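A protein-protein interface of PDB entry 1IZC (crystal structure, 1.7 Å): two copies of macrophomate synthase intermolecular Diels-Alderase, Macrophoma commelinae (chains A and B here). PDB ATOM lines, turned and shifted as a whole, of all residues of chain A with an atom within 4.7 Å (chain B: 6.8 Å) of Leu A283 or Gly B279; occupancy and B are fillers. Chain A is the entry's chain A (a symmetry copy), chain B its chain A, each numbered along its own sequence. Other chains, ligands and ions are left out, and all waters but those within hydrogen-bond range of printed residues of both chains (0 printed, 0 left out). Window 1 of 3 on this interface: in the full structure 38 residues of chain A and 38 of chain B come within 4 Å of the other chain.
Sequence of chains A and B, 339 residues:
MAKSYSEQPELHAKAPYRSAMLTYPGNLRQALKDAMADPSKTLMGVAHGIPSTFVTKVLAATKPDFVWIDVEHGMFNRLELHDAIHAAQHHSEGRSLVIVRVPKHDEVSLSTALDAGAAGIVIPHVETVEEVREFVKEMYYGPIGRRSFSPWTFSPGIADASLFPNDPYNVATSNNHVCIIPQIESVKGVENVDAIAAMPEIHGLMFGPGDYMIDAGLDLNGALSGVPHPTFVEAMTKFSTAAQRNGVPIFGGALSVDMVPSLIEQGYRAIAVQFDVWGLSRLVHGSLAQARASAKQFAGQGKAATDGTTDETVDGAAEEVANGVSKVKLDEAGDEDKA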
ATOM      1  N   GLY A 279      -7.549 -16.329  22.917  1.00  0.00           N
ATOM      2  CA  GLY A 279      -6.494 -15.393  22.556  1.00  0.00           C
ATOM      3  C   GLY A 279      -5.133 -15.829  23.082  1.00  0.00           C
ATOM      4  O   GLY A 279      -4.143 -15.862  22.344  1.00  0.00           O
ATOM      5  N   LEU A 280      -5.083 -16.157  24.367  1.00  0.00           N
ATOM      6  CA  LEU A 280      -3.830 -16.600  24.974  1.00  0.00           C
ATOM      7  C   LEU A 280      -3.387 -17.916  24.341  1.00  0.00           C
ATOM      8  O   LEU A 280      -2.211 -18.090  24.022  1.00  0.00           O
ATOM      9  CB  LEU A 280      -4.007 -16.788  26.482  1.00  0.00           C
ATOM     10  CG  LEU A 280      -2.798 -17.301  27.286  1.00  0.00           C
ATOM     11  CD1 LEU A 280      -1.647 -16.325  27.202  1.00  0.00           C
ATOM     12  CD2 LEU A 280      -3.219 -17.485  28.742  1.00  0.00           C
ATOM     13  N   SER A 281      -4.328 -18.838  24.162  1.00  0.00           N
ATOM     14  CA  SER A 281      -4.009 -20.139  23.567  1.00  0.00           C
ATOM     15  C   SER A 281      -3.364 -19.979  22.181  1.00  0.00           C
ATOM     16  O   SER A 281      -2.294 -20.537  21.900  1.00  0.00           O
ATOM     17  CB  SER A 281      -5.280 -20.985  23.469  1.00  0.00           C
ATOM     18  OG  SER A 281      -5.018 -22.253  22.903  1.00  0.00           O
ATOM     19  N   ARG A 282      -4.014 -19.204  21.313  1.00  0.00           N
ATOM     20  CA  ARG A 282      -3.506 -18.995  19.955  1.00  0.00           C
ATOM     21  C   ARG A 282      -2.182 -18.247  19.929  1.00  0.00           C
ATOM     22  O   ARG A 282      -1.307 -18.546  19.108  1.00  0.00           O
ATOM     23  CB  ARG A 282      -4.552 -18.249  19.113  1.00  0.00           C
ATOM     24  CG  ARG A 282      -5.855 -19.025  18.990  1.00  0.00           C
ATOM     25  CD  ARG A 282      -6.967 -18.218  18.313  1.00  0.00           C
ATOM     26  NE  ARG A 282      -8.189 -19.010  18.175  1.00  0.00           N
ATOM     27  CZ  ARG A 282      -9.293 -18.598  17.556  1.00  0.00           C
ATOM     28  NH1 ARG A 282      -9.345 -17.392  17.008  1.00  0.00           N
ATOM     29  NH2 ARG A 282     -10.347 -19.400  17.473  1.00  0.00           N
ATOM     30  N   LEU A 283      -2.026 -17.273  20.819  1.00  0.00           N
ATOM     31  CA  LEU A 283      -0.790 -16.511  20.880  1.00  0.00           C
ATOM     32  C   LEU A 283       0.386 -17.432  21.211  1.00  0.00           C
ATOM     33  O   LEU A 283       1.420 -17.413  20.536  1.00  0.00           O
ATOM     34  CB  LEU A 283      -0.893 -15.420  21.947  1.00  0.00           C
ATOM     35  CG  LEU A 283       0.391 -14.624  22.188  1.00  0.00           C
ATOM     36  CD1 LEU A 283       0.676 -13.742  20.978  1.00  0.00           C
ATOM     37  CD2 LEU A 283       0.242 -13.781  23.434  1.00  0.00           C
ATOM     38  N   VAL A 284       0.220 -18.242  22.252  1.00  0.00           N
ATOM     39  CA  VAL A 284       1.286 -19.142  22.670  1.00  0.00           C
ATOM     40  C   VAL A 284       1.522 -20.257  21.649  1.00  0.00           C
ATOM     41  O   VAL A 284       2.665 -20.521  21.264  1.00  0.00           O
ATOM     42  CB  VAL A 284       0.983 -19.742  24.071  1.00  0.00           C
ATOM     43  CG1 VAL A 284       2.061 -20.746  24.464  1.00  0.00           C
ATOM     44  CG2 VAL A 284       0.934 -18.619  25.111  1.00  0.00           C
ATOM     45  N   HIS A 285       0.449 -20.895  21.187  1.00  0.00           N
ATOM     46  CA  HIS A 285       0.592 -21.975  20.214  1.00  0.00           C
ATOM     47  C   HIS A 285       1.280 -21.471  18.942  1.00  0.00           C
ATOM     48  O   HIS A 285       2.138 -22.146  18.375  1.00  0.00           O
ATOM     49  CB  HIS A 285      -0.779 -22.538  19.849  1.00  0.00           C
ATOM     50  CG  HIS A 285      -0.721 -23.714  18.924  1.00  0.00           C
ATOM     51  ND1 HIS A 285      -0.530 -25.006  19.368  1.00  0.00           N
ATOM     52  CD2 HIS A 285      -0.840 -23.794  17.578  1.00  0.00           C
ATOM     53  CE1 HIS A 285      -0.542 -25.831  18.334  1.00  0.00           C
ATOM     54  NE2 HIS A 285      -0.729 -25.119  17.238  1.00  0.00           N
ATOM     55  N   GLY A 286       0.895 -20.277  18.497  1.00  0.00           N
ATOM     56  CA  GLY A 286       1.486 -19.718  17.294  1.00  0.00           C
ATOM     57  C   GLY A 286       2.952 -19.387  17.461  1.00  0.00           C
ATOM     58  O   GLY A 286       3.757 -19.613  16.542  1.00  0.00           O
ATOM     59  N   SER A 287       3.317 -18.856  18.630  1.00  0.00           N
ATOM     60  CA  SER A 287       4.706 -18.498  18.885  1.00  0.00           C
ATOM     61  C   SER A 287       5.560 -19.757  18.928  1.00  0.00           C
ATOM     62  O   SER A 287       6.675 -19.765  18.404  1.00  0.00           O
ATOM     63  CB  SER A 287       4.839 -17.728  20.200  1.00  0.00           C
ATOM     64  OG  SER A 287       4.142 -16.493  20.124  1.00  0.00           O
ATOM     65  N   THR B  62      -1.391 -26.096  24.816  1.00  0.00           N
ATOM     66  CA  THR B  62      -0.730 -25.663  23.577  1.00  0.00           C
ATOM     67  C   THR B  62       0.543 -26.481  23.347  1.00  0.00           C
ATOM     68  O   THR B  62       1.250 -26.279  22.359  1.00  0.00           O
ATOM     69  CB  THR B  62      -0.346 -24.162  23.584  1.00  0.00           C
ATOM     70  OG1 THR B  62       0.687 -23.926  24.549  1.00  0.00           O
ATOM     71  CG2 THR B  62      -1.584 -23.291  23.903  1.00  0.00           C
ATOM     72  N   VAL B 257       9.602 -13.536  18.545  1.00  0.00           N
ATOM     73  CA  VAL B 257       9.919 -14.874  18.081  1.00  0.00           C
ATOM     74  C   VAL B 257      10.949 -14.923  16.952  1.00  0.00           C
ATOM     75  O   VAL B 257      11.660 -15.918  16.810  1.00  0.00           O
ATOM     76  CB  VAL B 257       8.636 -15.627  17.683  1.00  0.00           C
ATOM     77  CG1 VAL B 257       8.935 -17.103  17.477  1.00  0.00           C
ATOM     78  CG2 VAL B 257       7.588 -15.468  18.789  1.00  0.00           C
ATOM     79  N   VAL B 273       9.367 -18.362  24.493  1.00  0.00           N
ATOM     80  CA  VAL B 273       8.965 -17.567  23.340  1.00  0.00           C
ATOM     81  C   VAL B 273       7.707 -16.733  23.516  1.00  0.00           C
ATOM     82  O   VAL B 273       7.295 -16.027  22.598  1.00  0.00           O
ATOM     83  CB  VAL B 273       8.816 -18.461  22.082  1.00  0.00           C
ATOM     84  CG1 VAL B 273      10.167 -19.130  21.758  1.00  0.00           C
ATOM     85  CG2 VAL B 273       7.736 -19.498  22.295  1.00  0.00           C
ATOM     86  N   GLN B 274       7.098 -16.818  24.690  1.00  0.00           N
ATOM     87  CA  GLN B 274       5.897 -16.040  24.986  1.00  0.00           C
ATOM     88  C   GLN B 274       5.833 -15.949  26.514  1.00  0.00           C
ATOM     89  O   GLN B 274       6.384 -16.799  27.217  1.00  0.00           O
ATOM     90  CB  GLN B 274       4.678 -16.757  24.395  1.00  0.00           C
ATOM     91  CG  GLN B 274       3.514 -15.882  23.936  1.00  0.00           C
ATOM     92  CD  GLN B 274       3.916 -14.500  23.453  1.00  0.00           C
ATOM     93  OE1 GLN B 274       4.048 -13.571  24.252  1.00  0.00           O
ATOM     94  NE2 GLN B 274       4.109 -14.355  22.148  1.00  0.00           N
ATOM     95  N   PHE B 275       5.188 -14.904  27.022  1.00  0.00           N
ATOM     96  CA  PHE B 275       5.074 -14.673  28.459  1.00  0.00           C
ATOM     97  C   PHE B 275       3.588 -14.430  28.673  1.00  0.00           C
ATOM     98  O   PHE B 275       2.989 -13.591  27.985  1.00  0.00           O
ATOM     99  CB  PHE B 275       5.935 -13.459  28.807  1.00  0.00           C
ATOM    100  CG  PHE B 275       7.259 -13.466  28.078  1.00  0.00           C
ATOM    101  CD1 PHE B 275       7.326 -13.096  26.730  1.00  0.00           C
ATOM    102  CD2 PHE B 275       8.401 -13.973  28.687  1.00  0.00           C
ATOM    103  CE1 PHE B 275       8.508 -13.241  25.997  1.00  0.00           C
ATOM    104  CE2 PHE B 275       9.593 -14.125  27.967  1.00  0.00           C
ATOM    105  CZ  PHE B 275       9.646 -13.761  26.618  1.00  0.00           C
ATOM    106  N   ASP B 276       2.975 -15.167  29.594  1.00  0.00           N
ATOM    107  CA  ASP B 276       1.544 -15.011  29.744  1.00  0.00           C
ATOM    108  C   ASP B 276       1.052 -13.618  30.093  1.00  0.00           C
ATOM    109  O   ASP B 276       0.138 -13.118  29.430  1.00  0.00           O
ATOM    110  CB  ASP B 276       0.948 -16.099  30.673  1.00  0.00           C
ATOM    111  CG  ASP B 276       1.458 -16.049  32.105  1.00  0.00           C
ATOM    112  OD1 ASP B 276       2.355 -15.251  32.444  1.00  0.00           O
ATOM    113  OD2 ASP B 276       0.919 -16.840  32.903  1.00  0.00           O
ATOM    114  N   VAL B 277       1.666 -12.949  31.065  1.00  0.00           N
ATOM    115  CA  VAL B 277       1.182 -11.618  31.433  1.00  0.00           C
ATOM    116  C   VAL B 277       1.355 -10.572  30.331  1.00  0.00           C
ATOM    117  O   VAL B 277       0.388  -9.918  29.908  1.00  0.00           O
ATOM    118  CB  VAL B 277       1.872 -11.107  32.719  1.00  0.00           C
ATOM    119  CG1 VAL B 277       1.404  -9.695  33.040  1.00  0.00           C
ATOM    120  CG2 VAL B 277       1.540 -12.036  33.876  1.00  0.00           C
ATOM    121  N   TRP B 278       2.586 -10.403  29.855  1.00  0.00           N
ATOM    122  CA  TRP B 278       2.815  -9.417  28.811  1.00  0.00           C
ATOM    123  C   TRP B 278       2.153  -9.804  27.503  1.00  0.00           C
ATOM    124  O   TRP B 278       1.670  -8.936  26.779  1.00  0.00           O
ATOM    125  CB  TRP B 278       4.318  -9.220  28.573  1.00  0.00           C
ATOM    126  CG  TRP B 278       5.002  -8.472  29.669  1.00  0.00           C
ATOM    127  CD1 TRP B 278       4.444  -8.016  30.830  1.00  0.00           C
ATOM    128  CD2 TRP B 278       6.380  -8.078  29.704  1.00  0.00           C
ATOM    129  NE1 TRP B 278       5.390  -7.364  31.587  1.00  0.00           N
ATOM    130  CE2 TRP B 278       6.587  -7.388  30.920  1.00  0.00           C
ATOM    131  CE3 TRP B 278       7.458  -8.241  28.825  1.00  0.00           C
ATOM    132  CZ2 TRP B 278       7.830  -6.863  31.282  1.00  0.00           C
ATOM    133  CZ3 TRP B 278       8.695  -7.719  29.184  1.00  0.00           C
ATOM    134  CH2 TRP B 278       8.870  -7.037  30.403  1.00  0.00           C
ATOM    135  N   GLY B 279       2.140 -11.102  27.202  1.00  0.00           N
ATOM    136  CA  GLY B 279       1.545 -11.577  25.961  1.00  0.00           C
ATOM    137  C   GLY B 279       0.056 -11.270  25.882  1.00  0.00           C
ATOM    138  O   GLY B 279      -0.435 -10.737  24.882  1.00  0.00           O
ATOM    139  N   LEU B 280      -0.667 -11.616  26.941  1.00  0.00           N
ATOM    140  CA  LEU B 280      -2.104 -11.358  26.977  1.00  0.00           C
ATOM    141  C   LEU B 280      -2.358  -9.853  26.954  1.00  0.00           C
ATOM    142  O   LEU B 280      -3.236  -9.380  26.231  1.00  0.00           O
ATOM    143  CB  LEU B 280      -2.722 -11.965  28.237  1.00  0.00           C
ATOM    144  CG  LEU B 280      -4.228 -11.751  28.471  1.00  0.00           C
ATOM    145  CD1 LEU B 280      -5.038 -12.384  27.361  1.00  0.00           C
ATOM    146  CD2 LEU B 280      -4.612 -12.371  29.812  1.00  0.00           C
ATOM    147  N   SER B 281      -1.594  -9.106  27.745  1.00  0.00           N
ATOM    148  CA  SER B 281      -1.759  -7.651  27.802  1.00  0.00           C
ATOM    149  C   SER B 281      -1.605  -7.013  26.413  1.00  0.00           C
ATOM    150  O   SER B 281      -2.466  -6.245  25.959  1.00  0.00           O
ATOM    151  CB  SER B 281      -0.739  -7.057  28.776  1.00  0.00           C
ATOM    152  OG  SER B 281      -0.865  -5.653  28.868  1.00  0.00           O
ATOM    153  N   ARG B 282      -0.511  -7.342  25.729  1.00  0.00           N
ATOM    154  CA  ARG B 282      -0.247  -6.779  24.403  1.00  0.00           C
ATOM    155  C   ARG B 282      -1.266  -7.221  23.361  1.00  0.00           C
ATOM    156  O   ARG B 282      -1.654  -6.435  22.489  1.00  0.00           O
ATOM    157  CB  ARG B 282       1.173  -7.153  23.946  1.00  0.00           C
ATOM    158  CG  ARG B 282       2.240  -6.611  24.884  1.00  0.00           C
ATOM    159  CD  ARG B 282       3.644  -7.127  24.548  1.00  0.00           C
ATOM    160  NE  ARG B 282       4.648  -6.553  25.443  1.00  0.00           N
ATOM    161  CZ  ARG B 282       5.959  -6.757  25.340  1.00  0.00           C
ATOM    162  NH1 ARG B 282       6.444  -7.529  24.378  1.00  0.00           N
ATOM    163  NH2 ARG B 282       6.791  -6.177  26.196  1.00  0.00           N
ATOM    164  N   LEU B 283      -1.700  -8.475  23.442  1.00  0.00           N
ATOM    165  CA  LEU B 283      -2.683  -8.983  22.500  1.00  0.00           C
ATOM    166  C   LEU B 283      -3.986  -8.190  22.613  1.00  0.00           C
ATOM    167  O   LEU B 283      -4.539  -7.726  21.609  1.00  0.00           O
ATOM    168  CB  LEU B 283      -2.966 -10.460  22.778  1.00  0.00           C
ATOM    169  CG  LEU B 283      -4.073 -11.080  21.924  1.00  0.00           C
ATOM    170  CD1 LEU B 283      -3.597 -11.200  20.482  1.00  0.00           C
ATOM    171  CD2 LEU B 283      -4.441 -12.439  22.475  1.00  0.00           C
ATOM    172  N   VAL B 284      -4.472  -8.031  23.840  1.00  0.00           N
ATOM    173  CA  VAL B 284      -5.720  -7.314  24.058  1.00  0.00           C
ATOM    174  C   VAL B 284      -5.577  -5.820  23.760  1.00  0.00           C
ATOM    175  O   VAL B 284      -6.406  -5.241  23.051  1.00  0.00           O
ATOM    176  CB  VAL B 284      -6.235  -7.534  25.507  1.00  0.00           C
ATOM    177  CG1 VAL B 284      -7.497  -6.714  25.752  1.00  0.00           C
ATOM    178  CG2 VAL B 284      -6.548  -9.017  25.722  1.00  0.00           C
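Hydrophobic or aromatic side chains of chain A within 4 Å of the printed part of chain B: Leu A283, Val A284 and His A285. Among the printed residues, 10 pairs touch across the chains. Among the printed residues, no Asp or Glu carboxylate lies within 4 Å of a Lys or Arg side-chain nitrogen of the other chain.
Gly A279 touches Leu B283, and with the chains exchanged Leu A283 touches Gly B279. Of the 10 pairs that touch across the chains among the printed residues, 2 have their exchanged pair printed and touching as well.
The backbone carbonyl oxygen (O) of Leu A283 is in hydrogen-bond range of the side-chain hydroxyl (OG) of Ser A287.
Leu A283 touches just these residues of chain B: Gln B274 (3.7 Å) and Gly B279 (3.4 Å). Gly B279 touches just one residue of chain A: Leu A283. Of the printed residues of chain A, Leu B283 touches Gly A279 (3.4 Å). Of the printed residues of chain A, Gln B274 touches Leu A283 (3.7 Å), Val A284 (3.9 Å) and Ser A287 (2.9 Å). Printed residues of chain B within 4 Å of Ser A281: Thr B62 (3.5 Å). Of the printed residues of chain B, Ser A287 touches Val B257, Val B273 and Gln B274. Of the printed residues of chain B, His A285 touches Thr B62. Arg A282 touches none of the printed residues of chain B. Gly A286 touches none of the printed residues of chain B. The nearest printed residue of chain A that does not touch Gly B279 is Leu A280 (5.5 Å). The nearest printed residue of chain B that does not touch Val A284 is Val B273 (5.3 Å).
O of Gly A279 touches CD2 of Leu B283, at 3.4 Å. O of Ser A281 touches CG2 of Thr B62, at 3.5 Å. Leu A283 touches Gln B274. Gly B279 touches Leu A283. Val A284 touches Thr B62 (CG1 to OG1, 3.5 Å). Val A284 touches Gln B274 (CG2 to CG, 3.9 Å). ND1 of His A285 touches O of Thr B62 (3.7 Å). CG1 of Val B257 touches O of Ser A287, at 3.6 Å. Val B273 touches Ser A287.
NE2 of Gln B274 sits at hydrogen-bond distance from OG of Ser A287.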
